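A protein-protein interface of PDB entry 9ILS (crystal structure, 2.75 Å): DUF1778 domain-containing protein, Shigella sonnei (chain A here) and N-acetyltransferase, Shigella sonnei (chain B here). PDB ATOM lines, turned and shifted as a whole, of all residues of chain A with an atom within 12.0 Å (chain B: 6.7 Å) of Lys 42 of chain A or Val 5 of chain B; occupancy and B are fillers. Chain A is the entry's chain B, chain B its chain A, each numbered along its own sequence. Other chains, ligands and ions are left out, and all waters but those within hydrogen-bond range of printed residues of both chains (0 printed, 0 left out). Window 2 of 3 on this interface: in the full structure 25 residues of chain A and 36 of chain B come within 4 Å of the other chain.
O of Val 5 of chain B is in hydrogen-bond range of N of Lys 42 of chain A (2.9 Å).
N of Thr 6 of chain B lies within hydrogen-bond range of O of Cys 50 of chain B (3.3 Å). O of Ile 49 of chain B is in hydrogen-bond range of N of Val 58 of chain B (2.8 Å). The backbone NH (N) of Ile 49 of chain B is in hydrogen-bond range of the backbone carbonyl oxygen (O) of Gly 59 of chain B (2.8 Å).
CG1 of Val 37 of chain A touches CD1 of Trp 107 of chain B, at 3.7 Å. Pro 39 of chain A touches Trp 107 of chain B. Glu 40 of chain A touches Trp 107 of chain B (N to CH2, 3.0 Å). Trp 41 of chain A touches Val 5 of chain B (C to O, 3.6 Å). Thr 6 of chain B touches Trp 41 of chain A. Ala 7 of chain B touches Trp 41 of chain A (CA to CB, 3.5 Å). Ile 49 of chain B touches Trp 41 of chain A (CG2 to CZ3, 3.4 Å). Trp 41 of chain A touches Trp 107 of chain B (CZ2 to O, 3.2 Å). Lys 42 of chain A touches Thr 6 of chain B. N of Lys 42 of chain A touches N of Ala 7 of chain B, 3.9 Å away.
Printed residues of chain B within 4 Å of Trp 41 of chain A: Val 5 (3.6 Å), Thr 6 (3.0 Å), Ala 7 (3.5 Å), Ile 49 (3.4 Å) and Trp 107 (3.2 Å). Lys 42 of chain A touches just these residues of chain B: Val 5 (2.9 Å), Thr 6 (3.6 Å) and Ala 7 (3.9 Å). No residue of chain A comes within 4 Å of Ile 3 of chain B. No residue of chain A comes within 4 Å of Asn 4 of chain B. Of chain A, only Trp 41 and Lys 42 come within 4 Å of Val 5 of chain B. Thr 6 of chain B touches just these residues of chain A: Trp 41 and Lys 42. Ala 7 of chain B touches two residues of chain A. No residue of chain A comes within 4 Å of Cys 50 of chain B. No residue of chain A comes within 4 Å of Leu 51 of chain B. No residue of chain A comes within 4 Å of Val 58 of chain B. Thr 99 of chain B touches none of the printed residues of chain A. No residue of chain A comes within 4 Å of Phe 104 of chain B. Printed residues of chain A within 4 Å of Trp 107 of chain B: Val 37 (3.7 Å), Pro 39 (3.4 Å), Glu 40 (3.0 Å) and Trp 41 (3.2 Å). The nearest residue of chain B that does not touch Lys 42 of chain A is Glu 52 of chain B (4.4 Å). The nearest residue of chain A that does not touch Val 5 of chain B is Glu 40 of chain A (4.02 Å). The nearest printed residue of chain B that does not touch Trp 41 of chain A is Phe 104 of chain B (5.0 Å).
Of the 14 printed residues of chain B, 5 touch a printed residue of chain A. Hydrophobic or aromatic side chains of chain A within 4 Å of the printed part of chain B: Val 37, Pro 39 and Trp 41.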
ATOM      1  N   VAL A  37     -29.576  -4.080 -26.769  1.00  0.00           N
ATOM      2  CA  VAL A  37     -28.346  -4.004 -25.999  1.00  0.00           C
ATOM      3  C   VAL A  37     -28.478  -5.005 -24.859  1.00  0.00           C
ATOM      4  O   VAL A  37     -29.138  -4.723 -23.853  1.00  0.00           O
ATOM      5  CB  VAL A  37     -28.097  -2.580 -25.464  1.00  0.00           C
ATOM      6  CG1 VAL A  37     -26.887  -2.550 -24.543  1.00  0.00           C
ATOM      7  CG2 VAL A  37     -27.996  -1.570 -26.606  1.00  0.00           C
ATOM      8  N   LYS A  38     -27.943  -6.219 -25.055  1.00  0.00           N
ATOM      9  CA  LYS A  38     -27.769  -7.187 -23.978  1.00  0.00           C
ATOM     10  C   LYS A  38     -26.369  -6.997 -23.425  1.00  0.00           C
ATOM     11  O   LYS A  38     -25.389  -7.355 -24.096  1.00  0.00           O
ATOM     12  CB  LYS A  38     -27.948  -8.624 -24.474  1.00  0.00           C
ATOM     13  N   PRO A  39     -26.211  -6.413 -22.241  1.00  0.00           N
ATOM     14  CA  PRO A  39     -24.873  -6.231 -21.667  1.00  0.00           C
ATOM     15  C   PRO A  39     -24.341  -7.513 -21.034  1.00  0.00           C
ATOM     16  O   PRO A  39     -25.093  -8.420 -20.681  1.00  0.00           O
ATOM     17  CB  PRO A  39     -25.090  -5.133 -20.612  1.00  0.00           C
ATOM     18  CG  PRO A  39     -26.593  -4.845 -20.593  1.00  0.00           C
ATOM     19  CD  PRO A  39     -27.278  -5.908 -21.365  1.00  0.00           C
ATOM     20  N   GLU A  40     -23.014  -7.578 -20.901  1.00  0.00           N
ATOM     21  CA  GLU A  40     -22.315  -8.715 -20.277  1.00  0.00           C
ATOM     22  C   GLU A  40     -21.641  -8.218 -18.998  1.00  0.00           C
ATOM     23  O   GLU A  40     -20.459  -7.869 -18.994  1.00  0.00           O
ATOM     24  CB  GLU A  40     -21.273  -9.365 -21.255  1.00  0.00           C
ATOM     25  N   TRP A  41     -22.398  -8.179 -17.908  1.00  0.00           N
ATOM     26  CA  TRP A  41     -21.841  -7.725 -16.644  1.00  0.00           C
ATOM     27  C   TRP A  41     -21.149  -8.872 -15.905  1.00  0.00           C
ATOM     28  O   TRP A  41     -21.450 -10.051 -16.110  1.00  0.00           O
ATOM     29  CB  TRP A  41     -22.942  -7.135 -15.766  1.00  0.00           C
ATOM     30  CG  TRP A  41     -23.738  -6.020 -16.389  1.00  0.00           C
ATOM     31  CD1 TRP A  41     -25.046  -6.068 -16.771  1.00  0.00           C
ATOM     32  CD2 TRP A  41     -23.287  -4.692 -16.672  1.00  0.00           C
ATOM     33  NE1 TRP A  41     -25.431  -4.862 -17.287  1.00  0.00           N
ATOM     34  CE2 TRP A  41     -24.369  -3.997 -17.232  1.00  0.00           C
ATOM     35  CE3 TRP A  41     -22.073  -4.028 -16.514  1.00  0.00           C
ATOM     36  CZ2 TRP A  41     -24.276  -2.671 -17.627  1.00  0.00           C
ATOM     37  CZ3 TRP A  41     -21.982  -2.716 -16.916  1.00  0.00           C
ATOM     38  CH2 TRP A  41     -23.076  -2.047 -17.456  1.00  0.00           C
ATOM     39  N   LYS A  42     -20.222  -8.517 -15.022  1.00  0.00           N
ATOM     40  CA  LYS A  42     -19.551  -9.554 -14.247  1.00  0.00           C
ATOM     41  C   LYS A  42     -19.661  -9.313 -12.751  1.00  0.00           C
ATOM     42  O   LYS A  42     -19.448 -10.224 -11.958  1.00  0.00           O
ATOM     43  CB  LYS A  42     -18.088  -9.660 -14.658  1.00  0.00           C
ATOM     44  N   ILE B   3     -11.685  -4.330 -21.870  1.00  0.00           N
ATOM     45  CA  ILE B   3     -12.046  -4.008 -20.495  1.00  0.00           C
ATOM     46  C   ILE B   3     -13.268  -4.844 -20.127  1.00  0.00           C
ATOM     47  O   ILE B   3     -14.205  -4.962 -20.924  1.00  0.00           O
ATOM     48  CB  ILE B   3     -12.327  -2.503 -20.324  1.00  0.00           C
ATOM     49  CG1 ILE B   3     -11.063  -1.689 -20.609  1.00  0.00           C
ATOM     50  CG2 ILE B   3     -12.820  -2.207 -18.909  1.00  0.00           C
ATOM     51  CD1 ILE B   3     -11.204  -0.709 -21.746  1.00  0.00           C
ATOM     52  N   ASN B   4     -13.243  -5.443 -18.937  1.00  0.00           N
ATOM     53  CA  ASN B   4     -14.339  -6.254 -18.415  1.00  0.00           C
ATOM     54  C   ASN B   4     -14.901  -5.596 -17.163  1.00  0.00           C
ATOM     55  O   ASN B   4     -14.142  -5.285 -16.241  1.00  0.00           O
ATOM     56  CB  ASN B   4     -13.867  -7.663 -18.062  1.00  0.00           C
ATOM     57  CG  ASN B   4     -13.924  -8.611 -19.232  1.00  0.00           C
ATOM     58  OD1 ASN B   4     -13.660  -9.805 -19.079  1.00  0.00           O
ATOM     59  ND2 ASN B   4     -14.262  -8.087 -20.416  1.00  0.00           N
ATOM     60  N   VAL B   5     -16.226  -5.424 -17.106  1.00  0.00           N
ATOM     61  CA  VAL B   5     -16.844  -4.632 -16.045  1.00  0.00           C
ATOM     62  C   VAL B   5     -17.904  -5.447 -15.306  1.00  0.00           C
ATOM     63  O   VAL B   5     -18.460  -6.422 -15.817  1.00  0.00           O
ATOM     64  CB  VAL B   5     -17.451  -3.313 -16.573  1.00  0.00           C
ATOM     65  CG1 VAL B   5     -16.346  -2.301 -16.870  1.00  0.00           C
ATOM     66  CG2 VAL B   5     -18.327  -3.559 -17.784  1.00  0.00           C
ATOM     67  N   THR B   6     -18.175  -5.023 -14.077  1.00  0.00           N
ATOM     68  CA  THR B   6     -19.151  -5.654 -13.201  1.00  0.00           C
ATOM     69  C   THR B   6     -20.510  -4.971 -13.326  1.00  0.00           C
ATOM     70  O   THR B   6     -20.643  -3.876 -13.882  1.00  0.00           O
ATOM     71  CB  THR B   6     -18.692  -5.607 -11.740  1.00  0.00           C
ATOM     72  OG1 THR B   6     -19.096  -4.364 -11.148  1.00  0.00           O
ATOM     73  CG2 THR B   6     -17.183  -5.720 -11.661  1.00  0.00           C
ATOM     74  N   ALA B   7     -21.521  -5.628 -12.762  1.00  0.00           N
ATOM     75  CA  ALA B   7     -22.895  -5.181 -12.915  1.00  0.00           C
ATOM     76  C   ALA B   7     -23.138  -3.881 -12.144  1.00  0.00           C
ATOM     77  O   ALA B   7     -22.645  -3.714 -11.023  1.00  0.00           O
ATOM     78  CB  ALA B   7     -23.859  -6.263 -12.431  1.00  0.00           C
ATOM     79  N   ILE B  49     -20.396   1.276 -12.098  1.00  0.00           N
ATOM     80  CA  ILE B  49     -19.791   0.023 -12.543  1.00  0.00           C
ATOM     81  C   ILE B  49     -18.289   0.120 -12.331  1.00  0.00           C
ATOM     82  O   ILE B  49     -17.702   1.209 -12.315  1.00  0.00           O
ATOM     83  CB  ILE B  49     -20.099  -0.336 -14.017  1.00  0.00           C
ATOM     84  CG1 ILE B  49     -19.959   0.875 -14.939  1.00  0.00           C
ATOM     85  CG2 ILE B  49     -21.494  -0.880 -14.127  1.00  0.00           C
ATOM     86  CD1 ILE B  49     -19.613   0.488 -16.361  1.00  0.00           C
ATOM     87  N   CYS B  50     -17.660  -1.030 -12.161  1.00  0.00           N
ATOM     88  CA  CYS B  50     -16.249  -1.049 -11.819  1.00  0.00           C
ATOM     89  C   CYS B  50     -15.490  -1.904 -12.824  1.00  0.00           C
ATOM     90  O   CYS B  50     -16.080  -2.498 -13.735  1.00  0.00           O
ATOM     91  CB  CYS B  50     -16.060  -1.540 -10.379  1.00  0.00           C
ATOM     92  SG  CYS B  50     -16.882  -0.453  -9.202  1.00  0.00           S
ATOM     93  N   LEU B  51     -14.165  -1.913 -12.685  1.00  0.00           N
ATOM     94  CA  LEU B  51     -13.345  -2.868 -13.414  1.00  0.00           C
ATOM     95  C   LEU B  51     -13.335  -4.201 -12.672  1.00  0.00           C
ATOM     96  O   LEU B  51     -13.288  -4.234 -11.441  1.00  0.00           O
ATOM     97  CB  LEU B  51     -11.923  -2.333 -13.587  1.00  0.00           C
ATOM     98  N   GLU B  52     -13.397  -5.300 -13.441  1.00  0.00           N
ATOM     99  CA  GLU B  52     -13.520  -6.653 -12.886  1.00  0.00           C
ATOM    100  C   GLU B  52     -12.432  -6.920 -11.847  1.00  0.00           C
ATOM    101  O   GLU B  52     -11.272  -6.554 -12.039  1.00  0.00           O
ATOM    102  CB  GLU B  52     -13.441  -7.703 -14.007  1.00  0.00           C
ATOM    103  CG  GLU B  52     -13.625  -9.175 -13.560  1.00  0.00           C
ATOM    104  CD  GLU B  52     -13.134 -10.206 -14.594  1.00  0.00           C
ATOM    105  OE1 GLU B  52     -11.953 -10.127 -15.002  1.00  0.00           O
ATOM    106  OE2 GLU B  52     -13.910 -11.113 -14.979  1.00  0.00           O
ATOM    107  N   VAL B  58     -15.690   2.845 -13.339  1.00  0.00           N
ATOM    108  CA  VAL B  58     -15.443   3.156 -14.744  1.00  0.00           C
ATOM    109  C   VAL B  58     -16.655   3.773 -15.446  1.00  0.00           C
ATOM    110  O   VAL B  58     -16.505   4.276 -16.569  1.00  0.00           O
ATOM    111  CB  VAL B  58     -14.944   1.904 -15.502  1.00  0.00           C
ATOM    112  CG1 VAL B  58     -13.450   1.701 -15.258  1.00  0.00           C
ATOM    113  CG2 VAL B  58     -15.678   0.677 -15.022  1.00  0.00           C
ATOM    114  N   GLY B  59     -17.831   3.793 -14.806  1.00  0.00           N
ATOM    115  CA  GLY B  59     -19.031   4.420 -15.347  1.00  0.00           C
ATOM    116  C   GLY B  59     -20.116   4.483 -14.290  1.00  0.00           C
ATOM    117  O   GLY B  59     -20.082   3.737 -13.304  1.00  0.00           O
ATOM    118  N   THR B  99     -12.533   3.687 -21.409  1.00  0.00           N
ATOM    119  CA  THR B  99     -13.421   2.751 -22.097  1.00  0.00           C
ATOM    120  C   THR B  99     -14.148   3.542 -23.175  1.00  0.00           C
ATOM    121  O   THR B  99     -14.951   4.430 -22.862  1.00  0.00           O
ATOM    122  CB  THR B  99     -14.429   2.104 -21.140  1.00  0.00           C
ATOM    123  OG1 THR B  99     -15.630   2.880 -21.127  1.00  0.00           O
ATOM    124  CG2 THR B  99     -13.873   2.016 -19.724  1.00  0.00           C
ATOM    125  N   PHE B 104     -19.910   1.307 -23.181  1.00  0.00           N
ATOM    126  CA  PHE B 104     -20.538   1.032 -21.897  1.00  0.00           C
ATOM    127  C   PHE B 104     -21.652   2.009 -21.574  1.00  0.00           C
ATOM    128  O   PHE B 104     -22.355   1.808 -20.578  1.00  0.00           O
ATOM    129  CB  PHE B 104     -19.488   1.055 -20.791  1.00  0.00           C
ATOM    130  CG  PHE B 104     -18.562  -0.123 -20.815  1.00  0.00           C
ATOM    131  CD1 PHE B 104     -18.917  -1.287 -21.478  1.00  0.00           C
ATOM    132  CD2 PHE B 104     -17.313  -0.041 -20.221  1.00  0.00           C
ATOM    133  CE1 PHE B 104     -18.062  -2.363 -21.514  1.00  0.00           C
ATOM    134  CE2 PHE B 104     -16.444  -1.106 -20.257  1.00  0.00           C
ATOM    135  CZ  PHE B 104     -16.817  -2.273 -20.905  1.00  0.00           C
ATOM    136  N   TRP B 107     -24.797   0.158 -22.340  1.00  0.00           N
ATOM    137  CA  TRP B 107     -24.922  -0.802 -21.250  1.00  0.00           C
ATOM    138  C   TRP B 107     -25.519  -0.168 -20.006  1.00  0.00           C
ATOM    139  O   TRP B 107     -26.292  -0.815 -19.284  1.00  0.00           O
ATOM    140  CB  TRP B 107     -23.555  -1.392 -20.911  1.00  0.00           C
ATOM    141  CG  TRP B 107     -23.109  -2.433 -21.837  1.00  0.00           C
ATOM    142  CD1 TRP B 107     -23.445  -2.555 -23.153  1.00  0.00           C
ATOM    143  CD2 TRP B 107     -22.237  -3.523 -21.538  1.00  0.00           C
ATOM    144  NE1 TRP B 107     -22.840  -3.662 -23.692  1.00  0.00           N
ATOM    145  CE2 TRP B 107     -22.088  -4.272 -22.722  1.00  0.00           C
ATOM    146  CE3 TRP B 107     -21.567  -3.944 -20.383  1.00  0.00           C
ATOM    147  CZ2 TRP B 107     -21.289  -5.417 -22.788  1.00  0.00           C
ATOM    148  CZ3 TRP B 107     -20.780  -5.087 -20.449  1.00  0.00           C
ATOM    149  CH2 TRP B 107     -20.648  -5.806 -21.644  1.00  0.00           C
